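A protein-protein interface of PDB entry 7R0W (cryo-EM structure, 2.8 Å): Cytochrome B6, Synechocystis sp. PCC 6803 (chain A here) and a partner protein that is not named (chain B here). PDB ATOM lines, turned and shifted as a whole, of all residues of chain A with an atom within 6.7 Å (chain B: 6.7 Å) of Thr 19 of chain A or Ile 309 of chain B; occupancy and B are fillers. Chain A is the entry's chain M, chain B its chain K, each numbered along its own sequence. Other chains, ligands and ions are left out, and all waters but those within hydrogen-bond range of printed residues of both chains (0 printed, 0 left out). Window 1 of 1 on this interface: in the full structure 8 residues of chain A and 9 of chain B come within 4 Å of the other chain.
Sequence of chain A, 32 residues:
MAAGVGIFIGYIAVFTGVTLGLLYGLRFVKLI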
ATOM      1  N   VAL A  14      24.617 -10.780 -13.832  1.00  0.00           N
ATOM      2  CA  VAL A  14      24.641  -9.612 -14.705  1.00  0.00           C
ATOM      3  C   VAL A  14      24.155  -8.395 -13.942  1.00  0.00           C
ATOM      4  O   VAL A  14      24.678  -7.291 -14.118  1.00  0.00           O
ATOM      5  CB  VAL A  14      23.849  -9.841 -16.011  1.00  0.00           C
ATOM      6  CG1 VAL A  14      24.192 -11.186 -16.639  1.00  0.00           C
ATOM      7  CG2 VAL A  14      22.333  -9.717 -15.797  1.00  0.00           C
ATOM      8  N   PHE A  15      23.110  -8.555 -13.127  1.00  0.00           N
ATOM      9  CA  PHE A  15      22.607  -7.394 -12.402  1.00  0.00           C
ATOM     10  C   PHE A  15      23.607  -6.899 -11.363  1.00  0.00           C
ATOM     11  O   PHE A  15      23.721  -5.690 -11.150  1.00  0.00           O
ATOM     12  CB  PHE A  15      21.239  -7.691 -11.809  1.00  0.00           C
ATOM     13  CG  PHE A  15      20.130  -7.312 -12.734  1.00  0.00           C
ATOM     14  CD1 PHE A  15      19.672  -8.197 -13.689  1.00  0.00           C
ATOM     15  CD2 PHE A  15      19.582  -6.043 -12.686  1.00  0.00           C
ATOM     16  CE1 PHE A  15      18.668  -7.833 -14.555  1.00  0.00           C
ATOM     17  CE2 PHE A  15      18.577  -5.676 -13.552  1.00  0.00           C
ATOM     18  CZ  PHE A  15      18.116  -6.574 -14.485  1.00  0.00           C
ATOM     19  N   THR A  16      24.341  -7.799 -10.706  1.00  0.00           N
ATOM     20  CA  THR A  16      25.395  -7.331  -9.813  1.00  0.00           C
ATOM     21  C   THR A  16      26.445  -6.585 -10.609  1.00  0.00           C
ATOM     22  O   THR A  16      26.958  -5.545 -10.172  1.00  0.00           O
ATOM     23  CB  THR A  16      26.056  -8.474  -9.042  1.00  0.00           C
ATOM     24  OG1 THR A  16      26.982  -9.163  -9.896  1.00  0.00           O
ATOM     25  CG2 THR A  16      25.052  -9.409  -8.454  1.00  0.00           C
ATOM     26  N   GLY A  17      26.772  -7.097 -11.791  1.00  0.00           N
ATOM     27  CA  GLY A  17      27.750  -6.416 -12.611  1.00  0.00           C
ATOM     28  C   GLY A  17      27.307  -5.026 -13.016  1.00  0.00           C
ATOM     29  O   GLY A  17      28.094  -4.083 -12.955  1.00  0.00           O
ATOM     30  N   VAL A  18      26.029  -4.859 -13.368  1.00  0.00           N
ATOM     31  CA  VAL A  18      25.585  -3.522 -13.738  1.00  0.00           C
ATOM     32  C   VAL A  18      25.498  -2.614 -12.514  1.00  0.00           C
ATOM     33  O   VAL A  18      25.877  -1.438 -12.575  1.00  0.00           O
ATOM     34  CB  VAL A  18      24.255  -3.565 -14.506  1.00  0.00           C
ATOM     35  CG1 VAL A  18      24.259  -4.684 -15.520  1.00  0.00           C
ATOM     36  CG2 VAL A  18      23.086  -3.732 -13.556  1.00  0.00           C
ATOM     37  N   THR A  19      25.065  -3.148 -11.367  1.00  0.00           N
ATOM     38  CA  THR A  19      24.930  -2.280 -10.203  1.00  0.00           C
ATOM     39  C   THR A  19      26.296  -1.776  -9.771  1.00  0.00           C
ATOM     40  O   THR A  19      26.453  -0.593  -9.453  1.00  0.00           O
ATOM     41  CB  THR A  19      24.214  -2.961  -9.034  1.00  0.00           C
ATOM     42  OG1 THR A  19      24.287  -2.115  -7.882  1.00  0.00           O
ATOM     43  CG2 THR A  19      24.869  -4.242  -8.680  1.00  0.00           C
ATOM     44  N   LEU A  20      27.310  -2.633  -9.817  1.00  0.00           N
ATOM     45  CA  LEU A  20      28.612  -2.233  -9.312  1.00  0.00           C
ATOM     46  C   LEU A  20      29.405  -1.494 -10.370  1.00  0.00           C
ATOM     47  O   LEU A  20      30.191  -0.601 -10.032  1.00  0.00           O
ATOM     48  CB  LEU A  20      29.388  -3.471  -8.876  1.00  0.00           C
ATOM     49  CG  LEU A  20      28.711  -4.311  -7.798  1.00  0.00           C
ATOM     50  CD1 LEU A  20      29.558  -5.526  -7.539  1.00  0.00           C
ATOM     51  CD2 LEU A  20      28.490  -3.508  -6.526  1.00  0.00           C
ATOM     52  N   GLY A  21      29.150  -1.788 -11.645  1.00  0.00           N
ATOM     53  CA  GLY A  21      29.687  -0.958 -12.699  1.00  0.00           C
ATOM     54  C   GLY A  21      29.206   0.464 -12.538  1.00  0.00           C
ATOM     55  O   GLY A  21      29.994   1.407 -12.551  1.00  0.00           O
ATOM     56  N   LEU A  22      27.902   0.628 -12.307  1.00  0.00           N
ATOM     57  CA  LEU A  22      27.347   1.965 -12.171  1.00  0.00           C
ATOM     58  C   LEU A  22      27.834   2.609 -10.884  1.00  0.00           C
ATOM     59  O   LEU A  22      28.163   3.797 -10.867  1.00  0.00           O
ATOM     60  CB  LEU A  22      25.822   1.893 -12.180  1.00  0.00           C
ATOM     61  CG  LEU A  22      25.129   1.619 -13.517  1.00  0.00           C
ATOM     62  CD1 LEU A  22      23.624   1.550 -13.306  1.00  0.00           C
ATOM     63  CD2 LEU A  22      25.486   2.639 -14.590  1.00  0.00           C
ATOM     64  N   LEU A  23      27.920   1.836  -9.802  1.00  0.00           N
ATOM     65  CA  LEU A  23      28.333   2.399  -8.525  1.00  0.00           C
ATOM     66  C   LEU A  23      29.748   2.952  -8.626  1.00  0.00           C
ATOM     67  O   LEU A  23      29.987   4.136  -8.364  1.00  0.00           O
ATOM     68  CB  LEU A  23      28.232   1.336  -7.429  1.00  0.00           C
ATOM     69  CG  LEU A  23      28.893   1.630  -6.078  1.00  0.00           C
ATOM     70  CD1 LEU A  23      27.973   2.456  -5.200  1.00  0.00           C
ATOM     71  CD2 LEU A  23      29.267   0.339  -5.373  1.00  0.00           C
ATOM     72  N   TYR A  24      30.702   2.108  -9.032  1.00  0.00           N
ATOM     73  CA  TYR A  24      32.083   2.562  -9.101  1.00  0.00           C
ATOM     74  C   TYR A  24      32.287   3.572 -10.223  1.00  0.00           C
ATOM     75  O   TYR A  24      33.145   4.451 -10.107  1.00  0.00           O
ATOM     76  CB  TYR A  24      33.014   1.364  -9.273  1.00  0.00           C
ATOM     77  CG  TYR A  24      33.236   0.593  -7.991  1.00  0.00           C
ATOM     78  CD1 TYR A  24      32.374  -0.427  -7.613  1.00  0.00           C
ATOM     79  CD2 TYR A  24      34.303   0.890  -7.156  1.00  0.00           C
ATOM     80  CE1 TYR A  24      32.573  -1.132  -6.442  1.00  0.00           C
ATOM     81  CE2 TYR A  24      34.509   0.192  -5.984  1.00  0.00           C
ATOM     82  CZ  TYR A  24      33.641  -0.817  -5.631  1.00  0.00           C
ATOM     83  OH  TYR A  24      33.846  -1.515  -4.463  1.00  0.00           O
ATOM     84  N   ILE B 304      12.310  -2.701 -13.774  1.00  0.00           N
ATOM     85  CA  ILE B 304      12.091  -2.438 -12.355  1.00  0.00           C
ATOM     86  C   ILE B 304      13.363  -2.704 -11.564  1.00  0.00           C
ATOM     87  O   ILE B 304      13.714  -1.948 -10.651  1.00  0.00           O
ATOM     88  CB  ILE B 304      10.920  -3.287 -11.828  1.00  0.00           C
ATOM     89  CG1 ILE B 304       9.587  -2.621 -12.164  1.00  0.00           C
ATOM     90  CG2 ILE B 304      11.048  -3.498 -10.319  1.00  0.00           C
ATOM     91  CD1 ILE B 304       8.384  -3.507 -11.936  1.00  0.00           C
ATOM     92  N   MET B 305      14.083  -3.770 -11.909  1.00  0.00           N
ATOM     93  CA  MET B 305      15.329  -4.072 -11.216  1.00  0.00           C
ATOM     94  C   MET B 305      16.338  -2.949 -11.413  1.00  0.00           C
ATOM     95  O   MET B 305      17.006  -2.516 -10.463  1.00  0.00           O
ATOM     96  CB  MET B 305      15.889  -5.392 -11.739  1.00  0.00           C
ATOM     97  CG  MET B 305      15.268  -6.622 -11.117  1.00  0.00           C
ATOM     98  SD  MET B 305      15.913  -8.140 -11.836  1.00  0.00           S
ATOM     99  CE  MET B 305      17.501  -8.267 -11.027  1.00  0.00           C
ATOM    100  N   LEU B 306      16.436  -2.436 -12.641  1.00  0.00           N
ATOM    101  CA  LEU B 306      17.420  -1.398 -12.908  1.00  0.00           C
ATOM    102  C   LEU B 306      17.010  -0.104 -12.220  1.00  0.00           C
ATOM    103  O   LEU B 306      17.858   0.632 -11.702  1.00  0.00           O
ATOM    104  CB  LEU B 306      17.585  -1.215 -14.417  1.00  0.00           C
ATOM    105  CG  LEU B 306      18.530  -0.134 -14.958  1.00  0.00           C
ATOM    106  CD1 LEU B 306      17.869   1.223 -15.058  1.00  0.00           C
ATOM    107  CD2 LEU B 306      19.806  -0.053 -14.127  1.00  0.00           C
ATOM    108  N   SER B 307      15.707   0.189 -12.198  1.00  0.00           N
ATOM    109  CA  SER B 307      15.247   1.381 -11.503  1.00  0.00           C
ATOM    110  C   SER B 307      15.488   1.267 -10.003  1.00  0.00           C
ATOM    111  O   SER B 307      15.754   2.275  -9.343  1.00  0.00           O
ATOM    112  CB  SER B 307      13.765   1.612 -11.789  1.00  0.00           C
ATOM    113  OG  SER B 307      12.957   0.891 -10.881  1.00  0.00           O
ATOM    114  N   GLN B 308      15.447   0.052  -9.454  1.00  0.00           N
ATOM    115  CA  GLN B 308      15.743  -0.107  -8.034  1.00  0.00           C
ATOM    116  C   GLN B 308      17.227   0.106  -7.771  1.00  0.00           C
ATOM    117  O   GLN B 308      17.613   0.704  -6.755  1.00  0.00           O
ATOM    118  CB  GLN B 308      15.318  -1.493  -7.554  1.00  0.00           C
ATOM    119  CG  GLN B 308      13.847  -1.620  -7.229  1.00  0.00           C
ATOM    120  CD  GLN B 308      13.378  -3.059  -7.227  1.00  0.00           C
ATOM    121  OE1 GLN B 308      14.186  -3.986  -7.253  1.00  0.00           O
ATOM    122  NE2 GLN B 308      12.069  -3.253  -7.193  1.00  0.00           N
ATOM    123  N   ILE B 309      18.074  -0.345  -8.699  1.00  0.00           N
ATOM    124  CA  ILE B 309      19.499  -0.051  -8.582  1.00  0.00           C
ATOM    125  C   ILE B 309      19.708   1.457  -8.574  1.00  0.00           C
ATOM    126  O   ILE B 309      20.448   2.002  -7.743  1.00  0.00           O
ATOM    127  CB  ILE B 309      20.288  -0.721  -9.719  1.00  0.00           C
ATOM    128  CG1 ILE B 309      20.293  -2.238  -9.546  1.00  0.00           C
ATOM    129  CG2 ILE B 309      21.713  -0.198  -9.752  1.00  0.00           C
ATOM    130  CD1 ILE B 309      20.521  -2.993 -10.836  1.00  0.00           C
ATOM    131  N   LEU B 310      19.059   2.155  -9.507  1.00  0.00           N
ATOM    132  CA  LEU B 310      19.245   3.596  -9.588  1.00  0.00           C
ATOM    133  C   LEU B 310      18.643   4.309  -8.387  1.00  0.00           C
ATOM    134  O   LEU B 310      19.126   5.380  -8.011  1.00  0.00           O
ATOM    135  CB  LEU B 310      18.622   4.133 -10.876  1.00  0.00           C
ATOM    136  CG  LEU B 310      19.304   3.700 -12.172  1.00  0.00           C
ATOM    137  CD1 LEU B 310      18.453   4.088 -13.367  1.00  0.00           C
ATOM    138  CD2 LEU B 310      20.693   4.301 -12.281  1.00  0.00           C
ATOM    139  N   LEU B 311      17.669   3.691  -7.718  1.00  0.00           N
ATOM    140  CA  LEU B 311      17.118   4.295  -6.513  1.00  0.00           C
ATOM    141  C   LEU B 311      18.101   4.174  -5.363  1.00  0.00           C
ATOM    142  O   LEU B 311      18.297   5.125  -4.596  1.00  0.00           O
ATOM    143  CB  LEU B 311      15.798   3.625  -6.143  1.00  0.00           C
ATOM    144  CG  LEU B 311      14.528   4.233  -6.728  1.00  0.00           C
ATOM    145  CD1 LEU B 311      13.368   3.269  -6.557  1.00  0.00           C
ATOM    146  CD2 LEU B 311      14.215   5.572  -6.092  1.00  0.00           C
ATOM    147  N   VAL B 312      18.777   3.029  -5.264  1.00  0.00           N
ATOM    148  CA  VAL B 312      19.758   2.898  -4.196  1.00  0.00           C
ATOM    149  C   VAL B 312      20.944   3.807  -4.479  1.00  0.00           C
ATOM    150  O   VAL B 312      21.550   4.355  -3.551  1.00  0.00           O
ATOM    151  CB  VAL B 312      20.201   1.438  -4.013  1.00  0.00           C
ATOM    152  CG1 VAL B 312      21.157   1.341  -2.839  1.00  0.00           C
ATOM    153  CG2 VAL B 312      19.000   0.541  -3.790  1.00  0.00           C
ATOM    154  N   LEU B 313      21.278   4.016  -5.753  1.00  0.00           N
ATOM    155  CA  LEU B 313      22.419   4.875  -6.054  1.00  0.00           C
ATOM    156  C   LEU B 313      22.078   6.341  -5.821  1.00  0.00           C
ATOM    157  O   LEU B 313      22.929   7.113  -5.356  1.00  0.00           O
ATOM    158  CB  LEU B 313      22.873   4.660  -7.495  1.00  0.00           C
ATOM    159  CG  LEU B 313      23.500   3.299  -7.790  1.00  0.00           C
ATOM    160  CD1 LEU B 313      23.632   3.099  -9.287  1.00  0.00           C
ATOM    161  CD2 LEU B 313      24.847   3.164  -7.107  1.00  0.00           C
ATOM    162  N   LYS B 314      20.826   6.731  -6.063  1.00  0.00           N
ATOM    163  CA  LYS B 314      20.429   8.089  -5.728  1.00  0.00           C
ATOM    164  C   LYS B 314      20.387   8.279  -4.220  1.00  0.00           C
ATOM    165  O   LYS B 314      20.697   9.369  -3.723  1.00  0.00           O
ATOM    166  CB  LYS B 314      19.074   8.417  -6.355  1.00  0.00           C
ATOM    167  CG  LYS B 314      18.531   9.794  -5.996  1.00  0.00           C
ATOM    168  CD  LYS B 314      19.394  10.903  -6.576  1.00  0.00           C
ATOM    169  CE  LYS B 314      19.356  12.149  -5.718  1.00  0.00           C
ATOM    170  NZ  LYS B 314      19.791  13.350  -6.476  1.00  0.00           N
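Met 305 of chain B touches Phe 15 of chain A. Leu 306 of chain B touches Phe 15 of chain A. Phe 15 of chain A touches Ile 309 of chain B (CD2 to CD1, 3.7 Å). Val 18 of chain A touches Ile 309 of chain B. Thr 19 of chain A touches Ile 309 of chain B (OG1 to CG2, 3.7 Å). Leu 313 of chain B touches Leu 22 of chain A (CD1 to CB, 3.8 Å). Leu 313 of chain B touches Leu 23 of chain A.
Of the printed residues of chain B, Val 18 of chain A touches Ile 309. Of the printed residues of chain B, Thr 19 of chain A touches Ile 309 (3.7 Å). Ile 309 of chain B touches three residues of chain A. Of the printed residues of chain A, Leu 313 of chain B touches Leu 22 (3.8 Å) and Leu 23 (3.7 Å). The nearest residue of chain B that does not touch Thr 19 of chain A is Leu 313 of chain B (4.6 Å). The nearest printed residue of chain A that does not touch Leu 306 of chain B is Leu 22 of chain A (4.2 Å).
Hydrophobic or aromatic side chains of chain B that line the printed part of chain A: Met 305, Ile 309 and Leu 313. Hydrophobic or aromatic side chains of chain A within 4 Å of the printed part of chain B: Phe 15, Val 18, Leu 22 and Leu 23. Among the printed residues, 7 pairs touch across the chains.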
